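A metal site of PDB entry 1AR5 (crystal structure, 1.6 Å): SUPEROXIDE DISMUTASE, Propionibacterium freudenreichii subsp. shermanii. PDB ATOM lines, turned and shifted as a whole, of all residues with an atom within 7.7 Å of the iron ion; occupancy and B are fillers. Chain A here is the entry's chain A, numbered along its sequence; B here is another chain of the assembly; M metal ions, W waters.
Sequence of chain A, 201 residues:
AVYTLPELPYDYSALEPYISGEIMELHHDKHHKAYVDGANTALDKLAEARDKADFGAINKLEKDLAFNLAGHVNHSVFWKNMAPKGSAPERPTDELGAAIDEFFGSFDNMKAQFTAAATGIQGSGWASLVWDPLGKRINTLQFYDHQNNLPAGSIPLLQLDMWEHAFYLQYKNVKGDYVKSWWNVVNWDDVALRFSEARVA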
ATOM      1  N   HIS A  27      -4.699  17.318  15.876  1.00  0.00           N
ATOM      2  CA  HIS A  27      -5.843  18.214  16.041  1.00  0.00           C
ATOM      3  C   HIS A  27      -6.956  17.947  15.035  1.00  0.00           C
ATOM      4  O   HIS A  27      -8.130  17.859  15.406  1.00  0.00           O
ATOM      5  CB  HIS A  27      -5.366  19.659  15.911  1.00  0.00           C
ATOM      6  CG  HIS A  27      -6.230  20.647  16.624  1.00  0.00           C
ATOM      7  ND1 HIS A  27      -5.981  21.996  16.603  1.00  0.00           N
ATOM      8  CD2 HIS A  27      -7.347  20.483  17.378  1.00  0.00           C
ATOM      9  CE1 HIS A  27      -6.891  22.628  17.318  1.00  0.00           C
ATOM     10  NE2 HIS A  27      -7.733  21.727  17.801  1.00  0.00           N
ATOM     11  N   HIS A  28      -6.589  17.806  13.771  1.00  0.00           N
ATOM     12  CA  HIS A  28      -7.562  17.557  12.724  1.00  0.00           C
ATOM     13  C   HIS A  28      -8.028  16.104  12.621  1.00  0.00           C
ATOM     14  O   HIS A  28      -9.215  15.808  12.714  1.00  0.00           O
ATOM     15  CB  HIS A  28      -7.009  18.020  11.378  1.00  0.00           C
ATOM     16  CG  HIS A  28      -7.918  17.725  10.225  1.00  0.00           C
ATOM     17  ND1 HIS A  28      -8.848  18.640   9.765  1.00  0.00           N
ATOM     18  CD2 HIS A  28      -8.055  16.632   9.445  1.00  0.00           C
ATOM     19  CE1 HIS A  28      -9.514  18.113   8.758  1.00  0.00           C
ATOM     20  NE2 HIS A  28      -9.064  16.895   8.546  1.00  0.00           N
ATOM     21  N   HIS A  31      -8.836  14.816  17.066  1.00  0.00           N
ATOM     22  CA  HIS A  31      -9.807  15.609  17.810  1.00  0.00           C
ATOM     23  C   HIS A  31     -11.045  16.039  17.026  1.00  0.00           C
ATOM     24  O   HIS A  31     -12.166  15.780  17.471  1.00  0.00           O
ATOM     25  CB  HIS A  31      -9.138  16.824  18.453  1.00  0.00           C
ATOM     26  CG  HIS A  31      -8.190  16.464  19.548  1.00  0.00           C
ATOM     27  ND1 HIS A  31      -6.819  16.498  19.402  1.00  0.00           N
ATOM     28  CD2 HIS A  31      -8.416  16.039  20.821  1.00  0.00           C
ATOM     29  CE1 HIS A  31      -6.248  16.101  20.518  1.00  0.00           C
ATOM     30  NE2 HIS A  31      -7.190  15.814  21.399  1.00  0.00           N
ATOM     31  N   HIS A  32     -10.852  16.673  15.871  1.00  0.00           N
ATOM     32  CA  HIS A  32     -11.985  17.118  15.075  1.00  0.00           C
ATOM     33  C   HIS A  32     -12.850  15.932  14.658  1.00  0.00           C
ATOM     34  O   HIS A  32     -14.074  15.998  14.728  1.00  0.00           O
ATOM     35  CB  HIS A  32     -11.522  17.920  13.855  1.00  0.00           C
ATOM     36  CG  HIS A  32     -12.617  18.723  13.215  1.00  0.00           C
ATOM     37  ND1 HIS A  32     -12.376  19.636  12.205  1.00  0.00           N
ATOM     38  CD2 HIS A  32     -13.960  18.750  13.429  1.00  0.00           C
ATOM     39  CE1 HIS A  32     -13.517  20.187  11.832  1.00  0.00           C
ATOM     40  NE2 HIS A  32     -14.490  19.672  12.557  1.00  0.00           N
ATOM     41  N   TYR A  35     -15.355  14.846  17.273  1.00  0.00           N
ATOM     42  CA  TYR A  35     -16.520  15.715  17.396  1.00  0.00           C
ATOM     43  C   TYR A  35     -17.568  15.423  16.338  1.00  0.00           C
ATOM     44  O   TYR A  35     -18.765  15.455  16.611  1.00  0.00           O
ATOM     45  CB  TYR A  35     -16.115  17.194  17.348  1.00  0.00           C
ATOM     46  CG  TYR A  35     -15.136  17.576  18.426  1.00  0.00           C
ATOM     47  CD1 TYR A  35     -15.306  17.121  19.730  1.00  0.00           C
ATOM     48  CD2 TYR A  35     -14.026  18.357  18.139  1.00  0.00           C
ATOM     49  CE1 TYR A  35     -14.388  17.436  20.727  1.00  0.00           C
ATOM     50  CE2 TYR A  35     -13.097  18.682  19.119  1.00  0.00           C
ATOM     51  CZ  TYR A  35     -13.280  18.222  20.417  1.00  0.00           C
ATOM     52  OH  TYR A  35     -12.375  18.547  21.398  1.00  0.00           O
ATOM     53  N   GLY A  71     -18.035  21.750  18.796  1.00  0.00           N
ATOM     54  CA  GLY A  71     -16.646  21.427  18.537  1.00  0.00           C
ATOM     55  C   GLY A  71     -16.381  21.313  17.041  1.00  0.00           C
ATOM     56  O   GLY A  71     -15.326  21.719  16.557  1.00  0.00           O
ATOM     57  N   ASN A  74     -16.719  25.030  15.517  1.00  0.00           N
ATOM     58  CA  ASN A  74     -15.543  25.806  15.912  1.00  0.00           C
ATOM     59  C   ASN A  74     -14.275  25.413  15.149  1.00  0.00           C
ATOM     60  O   ASN A  74     -13.546  26.282  14.674  1.00  0.00           O
ATOM     61  CB  ASN A  74     -15.296  25.662  17.422  1.00  0.00           C
ATOM     62  CG  ASN A  74     -16.374  26.333  18.267  1.00  0.00           C
ATOM     63  OD1 ASN A  74     -17.251  27.030  17.749  1.00  0.00           O
ATOM     64  ND2 ASN A  74     -16.312  26.122  19.581  1.00  0.00           N
ATOM     65  N   HIS A  75     -14.011  24.113  15.052  1.00  0.00           N
ATOM     66  CA  HIS A  75     -12.831  23.647  14.336  1.00  0.00           C
ATOM     67  C   HIS A  75     -12.923  23.870  12.828  1.00  0.00           C
ATOM     68  O   HIS A  75     -11.932  24.203  12.196  1.00  0.00           O
ATOM     69  CB  HIS A  75     -12.530  22.183  14.653  1.00  0.00           C
ATOM     70  CG  HIS A  75     -11.954  21.981  16.020  1.00  0.00           C
ATOM     71  ND1 HIS A  75     -12.728  21.728  17.131  1.00  0.00           N
ATOM     72  CD2 HIS A  75     -10.677  22.020  16.463  1.00  0.00           C
ATOM     73  CE1 HIS A  75     -11.958  21.626  18.193  1.00  0.00           C
ATOM     74  NE2 HIS A  75     -10.706  21.802  17.827  1.00  0.00           N
ATOM     75  N   PHE A  78     -12.062  27.328  12.332  1.00  0.00           N
ATOM     76  CA  PHE A  78     -10.655  27.476  12.692  1.00  0.00           C
ATOM     77  C   PHE A  78      -9.677  27.166  11.551  1.00  0.00           C
ATOM     78  O   PHE A  78      -8.762  27.931  11.293  1.00  0.00           O
ATOM     79  CB  PHE A  78     -10.357  26.581  13.916  1.00  0.00           C
ATOM     80  CG  PHE A  78      -9.001  26.814  14.531  1.00  0.00           C
ATOM     81  CD1 PHE A  78      -8.598  28.079  14.943  1.00  0.00           C
ATOM     82  CD2 PHE A  78      -8.139  25.740  14.739  1.00  0.00           C
ATOM     83  CE1 PHE A  78      -7.363  28.275  15.551  1.00  0.00           C
ATOM     84  CE2 PHE A  78      -6.899  25.923  15.348  1.00  0.00           C
ATOM     85  CZ  PHE A  78      -6.517  27.197  15.763  1.00  0.00           C
ATOM     86  N   TRP A  79      -9.907  26.047  10.862  1.00  0.00           N
ATOM     87  CA  TRP A  79      -9.049  25.636   9.753  1.00  0.00           C
ATOM     88  C   TRP A  79      -9.032  26.677   8.630  1.00  0.00           C
ATOM     89  O   TRP A  79      -7.975  27.051   8.134  1.00  0.00           O
ATOM     90  CB  TRP A  79      -9.504  24.299   9.165  1.00  0.00           C
ATOM     91  CG  TRP A  79      -9.625  23.165  10.155  1.00  0.00           C
ATOM     92  CD1 TRP A  79     -10.585  22.198  10.166  1.00  0.00           C
ATOM     93  CD2 TRP A  79      -8.765  22.881  11.273  1.00  0.00           C
ATOM     94  NE1 TRP A  79     -10.370  21.325  11.198  1.00  0.00           N
ATOM     95  CE2 TRP A  79      -9.268  21.721  11.895  1.00  0.00           C
ATOM     96  CE3 TRP A  79      -7.612  23.493  11.800  1.00  0.00           C
ATOM     97  CZ2 TRP A  79      -8.664  21.164  13.024  1.00  0.00           C
ATOM     98  CZ3 TRP A  79      -7.016  22.931  12.915  1.00  0.00           C
ATOM     99  CH2 TRP A  79      -7.545  21.776  13.516  1.00  0.00           C
ATOM    100  N   GLY A 125     -11.281  26.652  26.157  1.00  0.00           N
ATOM    101  CA  GLY A 125     -12.136  27.650  25.538  1.00  0.00           C
ATOM    102  C   GLY A 125     -11.636  28.217  24.221  1.00  0.00           C
ATOM    103  O   GLY A 125     -10.652  27.730  23.663  1.00  0.00           O
ATOM    104  N   TRP A 126     -12.331  29.238  23.742  1.00  0.00           N
ATOM    105  CA  TRP A 126     -11.993  29.902  22.485  1.00  0.00           C
ATOM    106  C   TRP A 126     -12.144  31.418  22.597  1.00  0.00           C
ATOM    107  O   TRP A 126     -12.937  31.917  23.392  1.00  0.00           O
ATOM    108  CB  TRP A 126     -12.959  29.468  21.365  1.00  0.00           C
ATOM    109  CG  TRP A 126     -12.964  28.030  21.046  1.00  0.00           C
ATOM    110  CD1 TRP A 126     -13.448  27.026  21.825  1.00  0.00           C
ATOM    111  CD2 TRP A 126     -12.484  27.407  19.850  1.00  0.00           C
ATOM    112  NE1 TRP A 126     -13.286  25.820  21.199  1.00  0.00           N
ATOM    113  CE2 TRP A 126     -12.693  26.028  19.981  1.00  0.00           C
ATOM    114  CE3 TRP A 126     -11.887  27.892  18.673  1.00  0.00           C
ATOM    115  CZ2 TRP A 126     -12.328  25.109  18.990  1.00  0.00           C
ATOM    116  CZ3 TRP A 126     -11.527  26.985  17.680  1.00  0.00           C
ATOM    117  CH2 TRP A 126     -11.752  25.604  17.849  1.00  0.00           C
ATOM    118  N   HIS A 146     -16.594  24.385  24.228  1.00  0.00           N
ATOM    119  CA  HIS A 146     -16.909  24.664  22.829  1.00  0.00           C
ATOM    120  C   HIS A 146     -18.263  25.338  22.692  1.00  0.00           C
ATOM    121  O   HIS A 146     -18.486  26.150  21.794  1.00  0.00           O
ATOM    122  CB  HIS A 146     -17.021  23.372  22.002  1.00  0.00           C
ATOM    123  CG  HIS A 146     -15.716  22.661  21.805  1.00  0.00           C
ATOM    124  ND1 HIS A 146     -15.585  21.297  21.985  1.00  0.00           N
ATOM    125  CD2 HIS A 146     -14.503  23.110  21.429  1.00  0.00           C
ATOM    126  CE1 HIS A 146     -14.350  20.948  21.729  1.00  0.00           C
ATOM    127  NE2 HIS A 146     -13.663  22.024  21.390  1.00  0.00           N
ATOM    128  N   ASP A 161      -8.485  28.656  18.891  1.00  0.00           N
ATOM    129  CA  ASP A 161      -8.613  27.521  19.802  1.00  0.00           C
ATOM    130  C   ASP A 161      -7.633  27.661  20.974  1.00  0.00           C
ATOM    131  O   ASP A 161      -6.422  27.663  20.773  1.00  0.00           O
ATOM    132  CB  ASP A 161      -8.345  26.214  19.039  1.00  0.00           C
ATOM    133  CG  ASP A 161      -8.747  24.976  19.825  1.00  0.00           C
ATOM    134  OD1 ASP A 161      -9.082  25.086  21.024  1.00  0.00           O
ATOM    135  OD2 ASP A 161      -8.739  23.868  19.241  1.00  0.00           O
ATOM    136  N   MET A 162      -8.173  27.796  22.190  1.00  0.00           N
ATOM    137  CA  MET A 162      -7.339  27.915  23.378  1.00  0.00           C
ATOM    138  C   MET A 162      -7.299  26.673  24.263  1.00  0.00           C
ATOM    139  O   MET A 162      -6.860  26.721  25.409  1.00  0.00           O
ATOM    140  CB  MET A 162      -7.704  29.161  24.196  1.00  0.00           C
ATOM    141  CG  MET A 162      -7.326  30.482  23.525  1.00  0.00           C
ATOM    142  SD  MET A 162      -5.587  30.588  22.980  1.00  0.00           S
ATOM    143  CE  MET A 162      -4.749  30.619  24.551  1.00  0.00           C
ATOM    144  N   TRP A 163      -7.796  25.551  23.726  1.00  0.00           N
ATOM    145  CA  TRP A 163      -7.733  24.281  24.446  1.00  0.00           C
ATOM    146  C   TRP A 163      -6.242  23.942  24.464  1.00  0.00           C
ATOM    147  O   TRP A 163      -5.529  24.253  23.505  1.00  0.00           O
ATOM    148  CB  TRP A 163      -8.482  23.179  23.693  1.00  0.00           C
ATOM    149  CG  TRP A 163      -9.967  23.174  23.871  1.00  0.00           C
ATOM    150  CD1 TRP A 163     -10.840  24.186  23.611  1.00  0.00           C
ATOM    151  CD2 TRP A 163     -10.758  22.070  24.328  1.00  0.00           C
ATOM    152  NE1 TRP A 163     -12.130  23.784  23.874  1.00  0.00           N
ATOM    153  CE2 TRP A 163     -12.106  22.492  24.318  1.00  0.00           C
ATOM    154  CE3 TRP A 163     -10.461  20.763  24.740  1.00  0.00           C
ATOM    155  CZ2 TRP A 163     -13.159  21.643  24.710  1.00  0.00           C
ATOM    156  CZ3 TRP A 163     -11.506  19.923  25.124  1.00  0.00           C
ATOM    157  CH2 TRP A 163     -12.839  20.373  25.111  1.00  0.00           C
ATOM    158  N   GLU A 164      -5.771  23.292  25.514  1.00  0.00           N
ATOM    159  CA  GLU A 164      -4.358  22.946  25.608  1.00  0.00           C
ATOM    160  C   GLU A 164      -3.820  22.063  24.483  1.00  0.00           C
ATOM    161  O   GLU A 164      -2.666  22.209  24.086  1.00  0.00           O
ATOM    162  CB  GLU A 164      -4.048  22.354  26.985  1.00  0.00           C
ATOM    163  CG  GLU A 164      -4.277  23.364  28.111  1.00  0.00           C
ATOM    164  CD  GLU A 164      -4.091  22.788  29.495  1.00  0.00           C
ATOM    165  OE1 GLU A 164      -4.505  21.646  29.733  1.00  0.00           O
ATOM    166  OE2 GLU A 164      -3.535  23.504  30.352  1.00  0.00           O
ATOM    167  N   HIS A 165      -4.652  21.208  23.906  1.00  0.00           N
ATOM    168  CA  HIS A 165      -4.208  20.346  22.810  1.00  0.00           C
ATOM    169  C   HIS A 165      -3.807  21.147  21.565  1.00  0.00           C
ATOM    170  O   HIS A 165      -3.098  20.633  20.692  1.00  0.00           O
ATOM    171  CB  HIS A 165      -5.270  19.297  22.442  1.00  0.00           C
ATOM    172  CG  HIS A 165      -6.531  19.847  21.850  1.00  0.00           C
ATOM    173  ND1 HIS A 165      -7.768  19.640  22.425  1.00  0.00           N
ATOM    174  CD2 HIS A 165      -6.758  20.558  20.728  1.00  0.00           C
ATOM    175  CE1 HIS A 165      -8.700  20.200  21.684  1.00  0.00           C
ATOM    176  NE2 HIS A 165      -8.111  20.768  20.638  1.00  0.00           N
ATOM    177  N   ALA A 166      -4.267  22.392  21.484  1.00  0.00           N
ATOM    178  CA  ALA A 166      -3.979  23.235  20.348  1.00  0.00           C
ATOM    179  C   ALA A 166      -2.569  23.839  20.351  1.00  0.00           C
ATOM    180  O   ALA A 166      -2.061  24.219  19.305  1.00  0.00           O
ATOM    181  CB  ALA A 166      -5.010  24.354  20.249  1.00  0.00           C
ATOM    182  N   TYR A 178       2.031  31.320  21.845  1.00  0.00           N
ATOM    183  CA  TYR A 178       1.147  30.687  20.874  1.00  0.00           C
ATOM    184  C   TYR A 178       0.254  31.734  20.200  1.00  0.00           C
ATOM    185  O   TYR A 178       0.136  31.751  18.970  1.00  0.00           O
ATOM    186  CB  TYR A 178       0.290  29.624  21.567  1.00  0.00           C
ATOM    187  CG  TYR A 178      -0.913  29.146  20.781  1.00  0.00           C
ATOM    188  CD1 TYR A 178      -0.769  28.503  19.548  1.00  0.00           C
ATOM    189  CD2 TYR A 178      -2.192  29.288  21.298  1.00  0.00           C
ATOM    190  CE1 TYR A 178      -1.877  28.008  18.863  1.00  0.00           C
ATOM    191  CE2 TYR A 178      -3.305  28.814  20.623  1.00  0.00           C
ATOM    192  CZ  TYR A 178      -3.143  28.172  19.408  1.00  0.00           C
ATOM    193  OH  TYR A 178      -4.250  27.680  18.756  1.00  0.00           O
ATOM    194  N   GLU B 164      -5.682  18.391  29.761  1.00  0.00           N
ATOM    195  CA  GLU B 164      -4.735  17.981  28.731  1.00  0.00           C
ATOM    196  C   GLU B 164      -3.254  18.200  29.082  1.00  0.00           C
ATOM    197  O   GLU B 164      -2.411  17.390  28.696  1.00  0.00           O
ATOM    198  CB  GLU B 164      -5.103  18.622  27.387  1.00  0.00           C
ATOM    199  CG  GLU B 164      -6.395  18.054  26.820  1.00  0.00           C
ATOM    200  CD  GLU B 164      -6.890  18.770  25.571  1.00  0.00           C
ATOM    201  OE1 GLU B 164      -6.725  19.998  25.456  1.00  0.00           O
ATOM    202  OE2 GLU B 164      -7.494  18.097  24.708  1.00  0.00           O
HETATM  203 FE    FE M   1      -9.185  22.104  19.308  1.00  0.00          FE
HETATM  204  O   HOH W   1     -10.601  22.465  20.818  1.00  0.00           O
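The iron ion is bound by OD2 of Asp 161 (1.8 Å), water W1 (2.1 Å), NE2 of His 27 (2.1 Å), NE2 of His 75 (2.1 Å) and NE2 of His 165 (2.2 Å).
Water W1 lies within hydrogen-bond range of the side-chain carboxylate of Asp 161 (3.0 Å) and a ring nitrogen (NE2) of His 146 (3.1 Å).
The backbone NH of Trp 163 lies within hydrogen-bond range of the side-chain carboxylate of Asp 161, 3.0 Å away. The backbone carbonyl oxygen (O) of Asp 161 sits at hydrogen-bond distance from the side-chain hydroxyl (OH) of Tyr 178. The backbone carbonyl oxygen of His 27 sits at hydrogen-bond distance from the backbone NH of His 32 (3.0 Å). The indole nitrogen (NE1) of Trp 79 lies close to the backbone carbonyl oxygen (O) of His 75 (3.4 Å). ND1 of His 75 lies within hydrogen-bond range of O of Gly 71 (2.7 Å). ND1 of His 165 sits at hydrogen-bond distance from OE2 of Glu 164 of chain B, 2.8 Å away.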
